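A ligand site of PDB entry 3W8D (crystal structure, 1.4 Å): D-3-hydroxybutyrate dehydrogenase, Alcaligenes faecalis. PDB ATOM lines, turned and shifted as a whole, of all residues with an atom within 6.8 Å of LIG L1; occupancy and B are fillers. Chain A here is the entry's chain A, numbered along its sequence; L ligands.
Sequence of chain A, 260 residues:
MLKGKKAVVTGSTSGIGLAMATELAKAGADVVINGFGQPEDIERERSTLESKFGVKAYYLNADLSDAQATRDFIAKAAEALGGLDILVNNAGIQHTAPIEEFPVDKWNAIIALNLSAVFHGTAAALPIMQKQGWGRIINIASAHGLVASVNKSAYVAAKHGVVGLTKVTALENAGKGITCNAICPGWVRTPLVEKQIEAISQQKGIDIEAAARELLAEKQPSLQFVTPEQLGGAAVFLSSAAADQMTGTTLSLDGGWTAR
Merely in contact with LIG L1: Trp 187 (3.5 Å), Leu 192 (3.6 Å) and Trp 257 (3.6 Å).
Hydrophobic or aromatic side chains that line LIG L1: His 144, Tyr 155, Trp 187, Leu 192 and Trp 257.
Nine residues have an atom within 4 Å of LIG L1: Gln 94, Ser 142, His 144, Lys 152, Tyr 155, Trp 187, Leu 192, Gln 196 and Trp 257.
Along chain A the residues within 4 Å of LIG L1 span positions 94 to 257.
The side-chain amide oxygen of Gln 220 lies within hydrogen-bond range of the backbone NH of Trp 187 (2.8 Å).
A ring nitrogen (NE2) of His 144 lies within hydrogen-bond range of the side-chain hydroxyl (OG) of Ser 149 (2.7 Å).
The side-chain hydroxyl (OG) of Ser 142 sits at hydrogen-bond distance from the backbone NH (N) of His 144.
The backbone carbonyl oxygen (O) of Leu 192 lies within hydrogen-bond range of the side-chain amide nitrogen (NE2) of Gln 196, at 3.3 Å.
The side-chain amide oxygen (OE1) of Gln 196 is in hydrogen-bond range of the side-chain amino group (NZ) of Lys 152, 2.8 Å away.
ND1 of His 144 sits at hydrogen-bond distance from O1 of LIG L1.
O3 of LIG L1 lies within hydrogen-bond range of NE2 of Gln 94 (3.0 Å).
N of Val 188 is in hydrogen-bond range of O14 of LG2 L2.
The backbone carbonyl oxygen of Val 188 lies within hydrogen-bond range of a nitrogen (N7) of LG2 L2 (3.1 Å).
OG of Ser 142 is in hydrogen-bond range of O1 of LIG L1, at 2.5 Å.
An oxygen (O12) of LG2 L2 lies within hydrogen-bond range of the side-chain amino group of Lys 159 (2.9 Å).
An oxygen (O13) of LG2 L2 lies within hydrogen-bond range of the side-chain hydroxyl (OH) of Tyr 155.
The side-chain amino group (NZ) of Lys 152 is in salt-bridge range of an oxygen (O4) of LIG L1 (2.7 Å).
The side-chain hydroxyl (OH) of Tyr 155 lies within hydrogen-bond range of an oxygen (O2) of LIG L1 (2.4 Å).
An oxygen (O3) of LIG L1 sits at hydrogen-bond distance from the side-chain amide nitrogen of Gln 196 (2.7 Å).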
ATOM      1  N   GLN A  94       9.113  11.390   9.076  1.00  0.00           N
ATOM      2  CA  GLN A  94      10.045  12.268   9.745  1.00  0.00           C
ATOM      3  C   GLN A  94      10.884  11.425  10.721  1.00  0.00           C
ATOM      4  O   GLN A  94      10.462  10.378  11.229  1.00  0.00           O
ATOM      5  CB  GLN A  94       9.230  13.320  10.547  1.00  0.00           C
ATOM      6  CG  GLN A  94      10.019  14.346  11.312  1.00  0.00           C
ATOM      7  CD  GLN A  94      10.964  15.157  10.422  1.00  0.00           C
ATOM      8  OE1 GLN A  94      11.982  14.614   9.971  1.00  0.00           O
ATOM      9  NE2 GLN A  94      10.637  16.418  10.150  1.00  0.00           N
ATOM     10  N   THR A  96      14.162  12.584  13.704  1.00  0.00           N
ATOM     11  CA  THR A  96      15.031  13.680  14.136  1.00  0.00           C
ATOM     12  C   THR A  96      16.265  13.155  14.873  1.00  0.00           C
ATOM     13  O   THR A  96      16.231  12.212  15.722  1.00  0.00           O
ATOM     14  CB  THR A  96      14.301  14.652  15.060  1.00  0.00           C
ATOM     15  OG1 THR A  96      14.103  13.979  16.291  1.00  0.00           O
ATOM     16  CG2 THR A  96      12.947  15.155  14.458  1.00  0.00           C
ATOM     17  N   ALA A 141       5.164  19.457   0.180  1.00  0.00           N
ATOM     18  CA  ALA A 141       6.506  19.694   0.640  1.00  0.00           C
ATOM     19  C   ALA A 141       6.460  20.062   2.086  1.00  0.00           C
ATOM     20  O   ALA A 141       5.904  19.272   2.899  1.00  0.00           O
ATOM     21  CB  ALA A 141       7.286  20.663  -0.297  1.00  0.00           C
ATOM     22  N   SER A 142       6.915  21.257   2.485  1.00  0.00           N
ATOM     23  CA  SER A 142       6.918  21.694   3.907  1.00  0.00           C
ATOM     24  C   SER A 142       7.560  23.066   3.931  1.00  0.00           C
ATOM     25  O   SER A 142       8.266  23.468   2.924  1.00  0.00           O
ATOM     26  CB  SER A 142       7.837  20.755   4.743  1.00  0.00           C
ATOM     27  OG  SER A 142       7.981  21.296   6.041  1.00  0.00           O
ATOM     28  N   ALA A 143       7.347  23.831   4.997  1.00  0.00           N
ATOM     29  CA  ALA A 143       8.260  24.948   5.240  1.00  0.00           C
ATOM     30  C   ALA A 143       9.723  24.506   5.134  1.00  0.00           C
ATOM     31  O   ALA A 143      10.581  25.284   4.713  1.00  0.00           O
ATOM     32  CB  ALA A 143       7.948  25.518   6.685  1.00  0.00           C
ATOM     33  N   HIS A 144      10.018  23.228   5.503  1.00  0.00           N
ATOM     34  CA  HIS A 144      11.325  22.620   5.434  1.00  0.00           C
ATOM     35  C   HIS A 144      11.752  22.269   4.037  1.00  0.00           C
ATOM     36  O   HIS A 144      12.883  21.778   3.855  1.00  0.00           O
ATOM     37  CB  HIS A 144      11.415  21.441   6.375  1.00  0.00           C
ATOM     38  CG  HIS A 144      11.563  21.859   7.805  1.00  0.00           C
ATOM     39  ND1 HIS A 144      10.664  21.418   8.786  1.00  0.00           N
ATOM     40  CD2 HIS A 144      12.426  22.708   8.377  1.00  0.00           C
ATOM     41  CE1 HIS A 144      11.059  21.971   9.942  1.00  0.00           C
ATOM     42  NE2 HIS A 144      12.102  22.773   9.729  1.00  0.00           N
ATOM     43  N   GLY A 145      10.995  22.640   3.001  1.00  0.00           N
ATOM     44  CA  GLY A 145      11.483  22.682   1.626  1.00  0.00           C
ATOM     45  C   GLY A 145      12.045  24.020   1.269  1.00  0.00           C
ATOM     46  O   GLY A 145      12.585  24.147   0.132  1.00  0.00           O
ATOM     47  N   SER A 149      15.742  23.378   9.868  1.00  0.00           N
ATOM     48  CA  SER A 149      15.854  23.325  11.317  1.00  0.00           C
ATOM     49  C   SER A 149      16.886  22.292  11.661  1.00  0.00           C
ATOM     50  O   SER A 149      17.208  21.427  10.846  1.00  0.00           O
ATOM     51  CB  SER A 149      14.571  22.841  11.987  1.00  0.00           C
ATOM     52  OG  SER A 149      13.523  23.788  11.760  1.00  0.00           O
ATOM     53  N   LYS A 152      17.103  17.676  11.370  1.00  0.00           N
ATOM     54  CA  LYS A 152      16.202  17.216  10.318  1.00  0.00           C
ATOM     55  C   LYS A 152      16.839  17.170   8.940  1.00  0.00           C
ATOM     56  O   LYS A 152      16.220  17.430   7.916  1.00  0.00           O
ATOM     57  CB  LYS A 152      14.935  18.116  10.277  1.00  0.00           C
ATOM     58  CG  LYS A 152      14.004  17.836  11.523  1.00  0.00           C
ATOM     59  CD  LYS A 152      12.970  18.828  11.695  1.00  0.00           C
ATOM     60  CE  LYS A 152      12.085  18.404  12.890  1.00  0.00           C
ATOM     61  NZ  LYS A 152      10.969  19.422  13.158  1.00  0.00           N
ATOM     62  N   TYR A 155      15.031  15.038   6.135  1.00  0.00           N
ATOM     63  CA  TYR A 155      13.742  15.547   5.769  1.00  0.00           C
ATOM     64  C   TYR A 155      13.855  16.925   5.014  1.00  0.00           C
ATOM     65  O   TYR A 155      13.168  17.114   3.992  1.00  0.00           O
ATOM     66  CB  TYR A 155      12.960  15.724   7.072  1.00  0.00           C
ATOM     67  CG  TYR A 155      11.508  16.203   6.882  1.00  0.00           C
ATOM     68  CD1 TYR A 155      11.172  17.558   6.903  1.00  0.00           C
ATOM     69  CD2 TYR A 155      10.479  15.260   6.723  1.00  0.00           C
ATOM     70  CE1 TYR A 155       9.808  17.929   6.728  1.00  0.00           C
ATOM     71  CE2 TYR A 155       9.158  15.596   6.634  1.00  0.00           C
ATOM     72  CZ  TYR A 155       8.834  16.922   6.648  1.00  0.00           C
ATOM     73  OH  TYR A 155       7.535  17.283   6.470  1.00  0.00           O
ATOM     74  N   LYS A 159      12.651  17.526   1.292  1.00  0.00           N
ATOM     75  CA  LYS A 159      11.610  18.506   0.974  1.00  0.00           C
ATOM     76  C   LYS A 159      12.126  19.606   0.056  1.00  0.00           C
ATOM     77  O   LYS A 159      11.380  20.076  -0.813  1.00  0.00           O
ATOM     78  CB  LYS A 159      11.017  19.086   2.292  1.00  0.00           C
ATOM     79  CG  LYS A 159      10.196  18.064   3.083  1.00  0.00           C
ATOM     80  CD  LYS A 159       9.025  17.446   2.274  1.00  0.00           C
ATOM     81  CE  LYS A 159       8.017  16.695   3.241  1.00  0.00           C
ATOM     82  NZ  LYS A 159       6.900  16.154   2.536  1.00  0.00           N
ATOM     83  N   PRO A 185       3.418  23.317   4.180  1.00  0.00           N
ATOM     84  CA  PRO A 185       2.829  23.584   5.502  1.00  0.00           C
ATOM     85  C   PRO A 185       3.880  23.866   6.536  1.00  0.00           C
ATOM     86  O   PRO A 185       4.988  23.328   6.501  1.00  0.00           O
ATOM     87  CB  PRO A 185       2.036  22.281   5.912  1.00  0.00           C
ATOM     88  CG  PRO A 185       1.886  21.516   4.564  1.00  0.00           C
ATOM     89  CD  PRO A 185       3.213  21.877   3.816  1.00  0.00           C
ATOM     90  N   GLY A 186       3.429  24.738   7.480  1.00  0.00           N
ATOM     91  CA  GLY A 186       4.086  24.782   8.783  1.00  0.00           C
ATOM     92  C   GLY A 186       3.549  23.650   9.658  1.00  0.00           C
ATOM     93  O   GLY A 186       3.066  22.624   9.171  1.00  0.00           O
ATOM     94  N   TRP A 187       3.646  23.829  10.986  1.00  0.00           N
ATOM     95  CA  TRP A 187       3.152  22.744  11.871  1.00  0.00           C
ATOM     96  C   TRP A 187       1.671  22.489  11.764  1.00  0.00           C
ATOM     97  O   TRP A 187       0.867  23.438  11.763  1.00  0.00           O
ATOM     98  CB  TRP A 187       3.362  23.150  13.381  1.00  0.00           C
ATOM     99  CG  TRP A 187       4.737  23.300  13.862  1.00  0.00           C
ATOM    100  CD1 TRP A 187       5.324  24.474  14.266  1.00  0.00           C
ATOM    101  CD2 TRP A 187       5.736  22.286  14.006  1.00  0.00           C
ATOM    102  NE1 TRP A 187       6.611  24.206  14.765  1.00  0.00           N
ATOM    103  CE2 TRP A 187       6.871  22.894  14.579  1.00  0.00           C
ATOM    104  CE3 TRP A 187       5.762  20.919  13.791  1.00  0.00           C
ATOM    105  CZ2 TRP A 187       8.080  22.152  14.841  1.00  0.00           C
ATOM    106  CZ3 TRP A 187       6.895  20.185  14.106  1.00  0.00           C
ATOM    107  CH2 TRP A 187       7.989  20.797  14.648  1.00  0.00           C
ATOM    108  N   VAL A 188       1.306  21.211  11.644  1.00  0.00           N
ATOM    109  CA  VAL A 188      -0.075  20.678  11.521  1.00  0.00           C
ATOM    110  C   VAL A 188      -0.093  19.561  12.565  1.00  0.00           C
ATOM    111  O   VAL A 188       0.810  18.697  12.588  1.00  0.00           O
ATOM    112  CB  VAL A 188      -0.297  20.066  10.139  1.00  0.00           C
ATOM    113  CG1 VAL A 188      -1.722  19.546  10.013  1.00  0.00           C
ATOM    114  CG2 VAL A 188      -0.011  21.104   9.029  1.00  0.00           C
ATOM    115  N   LEU A 192       2.670  12.720  12.996  1.00  0.00           N
ATOM    116  CA  LEU A 192       4.054  13.020  12.674  1.00  0.00           C
ATOM    117  C   LEU A 192       4.599  14.116  13.634  1.00  0.00           C
ATOM    118  O   LEU A 192       5.776  14.117  13.972  1.00  0.00           O
ATOM    119  CB  LEU A 192       4.094  13.462  11.180  1.00  0.00           C
ATOM    120  CG  LEU A 192       5.497  13.871  10.600  1.00  0.00           C
ATOM    121  CD1 LEU A 192       5.411  13.563   9.169  1.00  0.00           C
ATOM    122  CD2 LEU A 192       5.875  15.431  10.863  1.00  0.00           C
ATOM    123  N   VAL A 193       3.741  15.079  14.055  1.00  0.00           N
ATOM    124  CA  VAL A 193       4.079  16.195  14.941  1.00  0.00           C
ATOM    125  C   VAL A 193       3.860  15.777  16.391  1.00  0.00           C
ATOM    126  O   VAL A 193       4.580  16.234  17.242  1.00  0.00           O
ATOM    127  CB  VAL A 193       3.294  17.429  14.503  1.00  0.00           C
ATOM    128  CG1 VAL A 193       3.278  18.559  15.540  1.00  0.00           C
ATOM    129  CG2 VAL A 193       3.906  17.916  13.139  1.00  0.00           C
ATOM    130  N   GLN A 196       6.838  14.601  18.044  1.00  0.00           N
ATOM    131  CA  GLN A 196       7.791  15.600  18.399  1.00  0.00           C
ATOM    132  C   GLN A 196       7.364  16.400  19.611  1.00  0.00           C
ATOM    133  O   GLN A 196       8.165  16.809  20.423  1.00  0.00           O
ATOM    134  CB  GLN A 196       8.005  16.607  17.235  1.00  0.00           C
ATOM    135  CG  GLN A 196       8.534  15.843  16.023  1.00  0.00           C
ATOM    136  CD  GLN A 196       8.784  16.737  14.787  1.00  0.00           C
ATOM    137  OE1 GLN A 196       9.572  17.645  14.882  1.00  0.00           O
ATOM    138  NE2 GLN A 196       8.003  16.517  13.747  1.00  0.00           N
ATOM    139  N   GLN A 220       6.410  29.341  14.527  1.00  0.00           N
ATOM    140  CA  GLN A 220       5.178  29.663  13.798  1.00  0.00           C
ATOM    141  C   GLN A 220       4.529  30.905  14.458  1.00  0.00           C
ATOM    142  O   GLN A 220       3.859  30.782  15.468  1.00  0.00           O
ATOM    143  CB  GLN A 220       4.296  28.413  13.878  1.00  0.00           C
ATOM    144  CG  GLN A 220       3.037  28.461  12.963  1.00  0.00           C
ATOM    145  CD  GLN A 220       2.825  27.105  12.382  1.00  0.00           C
ATOM    146  OE1 GLN A 220       3.779  26.493  11.848  1.00  0.00           O
ATOM    147  NE2 GLN A 220       1.587  26.571  12.401  1.00  0.00           N
ATOM    148  N   TRP A 257       5.912  31.314   9.336  1.00  0.00           N
ATOM    149  CA  TRP A 257       7.245  30.703   9.580  1.00  0.00           C
ATOM    150  C   TRP A 257       8.326  31.253   8.626  1.00  0.00           C
ATOM    151  O   TRP A 257       9.406  31.673   9.042  1.00  0.00           O
ATOM    152  CB  TRP A 257       7.060  29.190   9.449  1.00  0.00           C
ATOM    153  CG  TRP A 257       8.264  28.276   9.734  1.00  0.00           C
ATOM    154  CD1 TRP A 257       9.561  28.481   9.433  1.00  0.00           C
ATOM    155  CD2 TRP A 257       8.131  26.970  10.271  1.00  0.00           C
ATOM    156  NE1 TRP A 257      10.322  27.335   9.816  1.00  0.00           N
ATOM    157  CE2 TRP A 257       9.432  26.399  10.337  1.00  0.00           C
ATOM    158  CE3 TRP A 257       7.033  26.205  10.715  1.00  0.00           C
ATOM    159  CZ2 TRP A 257       9.678  25.140  10.881  1.00  0.00           C
ATOM    160  CZ3 TRP A 257       7.243  24.941  11.278  1.00  0.00           C
ATOM    161  CH2 TRP A 257       8.567  24.385  11.282  1.00  0.00           C
HETATM  162  C1  LIG L   1       7.305  19.311   8.988  1.00  0.00           C
HETATM  163  O1  LIG L   1       8.039  20.006   8.218  1.00  0.00           O
HETATM  164  O2  LIG L   1       6.810  18.241   8.598  1.00  0.00           O
HETATM  165  C2  LIG L   1       7.108  19.646  10.425  1.00  0.00           C
HETATM  166  C3  LIG L   1       6.986  21.203  10.555  1.00  0.00           C
HETATM  167  C4  LIG L   1       8.372  19.119  11.015  1.00  0.00           C
HETATM  168  O3  LIG L   1       8.411  17.942  11.465  1.00  0.00           O
HETATM  169  O4  LIG L   1       9.369  19.847  11.067  1.00  0.00           O
HETATM  170  P1  LG2 L   2       0.856  11.300   9.027  1.00  0.00           P
HETATM  171  O1  LG2 L   2       1.877  10.512   9.675  1.00  0.00           O
HETATM  172  O2  LG2 L   2      -0.294  11.612   9.890  1.00  0.00           O
HETATM  173  O3  LG2 L   2       0.422  10.614   7.667  1.00  0.00           O
HETATM  174  C1  LG2 L   2       1.434   9.977   6.817  1.00  0.00           C
HETATM  175  C2  LG2 L   2       0.586   9.251   5.774  1.00  0.00           C
HETATM  176  O4  LG2 L   2       1.587   8.603   4.908  1.00  0.00           O
HETATM  177  C3  LG2 L   2      -0.149   8.053   6.416  1.00  0.00           C
HETATM  178  O5  LG2 L   2      -1.294   7.772   5.625  1.00  0.00           O
HETATM  179  C4  LG2 L   2       0.860   6.914   6.324  1.00  0.00           C
HETATM  180  O6  LG2 L   2       0.241   5.594   6.381  1.00  0.00           O
HETATM  181  C5  LG2 L   2       1.434   7.142   4.944  1.00  0.00           C
HETATM  182  N1  LG2 L   2       2.655   6.474   4.663  1.00  0.00           N
HETATM  183  C6  LG2 L   2       3.774   6.385   5.506  1.00  0.00           C
HETATM  184  N2  LG2 L   2       4.729   5.632   4.961  1.00  0.00           N
HETATM  185  C7  LG2 L   2       4.251   5.241   3.713  1.00  0.00           C
HETATM  186  C8  LG2 L   2       4.733   4.435   2.681  1.00  0.00           C
HETATM  187  N3  LG2 L   2       6.003   3.890   2.718  1.00  0.00           N
HETATM  188  N4  LG2 L   2       3.923   4.283   1.593  1.00  0.00           N
HETATM  189  C9  LG2 L   2       2.697   4.785   1.521  1.00  0.00           C
HETATM  190  N5  LG2 L   2       2.125   5.547   2.490  1.00  0.00           N
HETATM  191  C10 LG2 L   2       2.969   5.777   3.526  1.00  0.00           C
HETATM  192  O7  LG2 L   2       1.636  12.642   8.597  1.00  0.00           O
HETATM  193  P2  LG2 L   2       1.197  14.054   8.019  1.00  0.00           P
HETATM  194  O8  LG2 L   2       1.665  15.037   8.993  1.00  0.00           O
HETATM  195  O9  LG2 L   2      -0.177  14.065   7.586  1.00  0.00           O
HETATM  196  O10 LG2 L   2       2.133  14.123   6.739  1.00  0.00           O
HETATM  197  C11 LG2 L   2       1.646  14.167   5.368  1.00  0.00           C
HETATM  198  C12 LG2 L   2       2.632  14.992   4.587  1.00  0.00           C
HETATM  199  O11 LG2 L   2       2.651  16.381   5.081  1.00  0.00           O
HETATM  200  C13 LG2 L   2       4.055  14.420   4.653  1.00  0.00           C
HETATM  201  O12 LG2 L   2       4.670  14.552   3.315  1.00  0.00           O
HETATM  202  C14 LG2 L   2       4.773  15.381   5.582  1.00  0.00           C
HETATM  203  O13 LG2 L   2       6.161  15.458   5.282  1.00  0.00           O
HETATM  204  C15 LG2 L   2       4.036  16.681   5.241  1.00  0.00           C
HETATM  205  N6  LG2 L   2       4.143  17.781   6.213  1.00  0.00           N
HETATM  206  C16 LG2 L   2       3.562  17.646   7.468  1.00  0.00           C
HETATM  207  C17 LG2 L   2       3.634  18.670   8.372  1.00  0.00           C
HETATM  208  C18 LG2 L   2       3.066  18.596   9.728  1.00  0.00           C
HETATM  209  O14 LG2 L   2       3.318  19.559  10.534  1.00  0.00           O
HETATM  210  N7  LG2 L   2       2.280  17.568  10.061  1.00  0.00           N
HETATM  211  C19 LG2 L   2       4.235  19.893   8.021  1.00  0.00           C
HETATM  212  C20 LG2 L   2       4.792  20.025   6.694  1.00  0.00           C
HETATM  213  C21 LG2 L   2       4.719  18.971   5.753  1.00  0.00           C
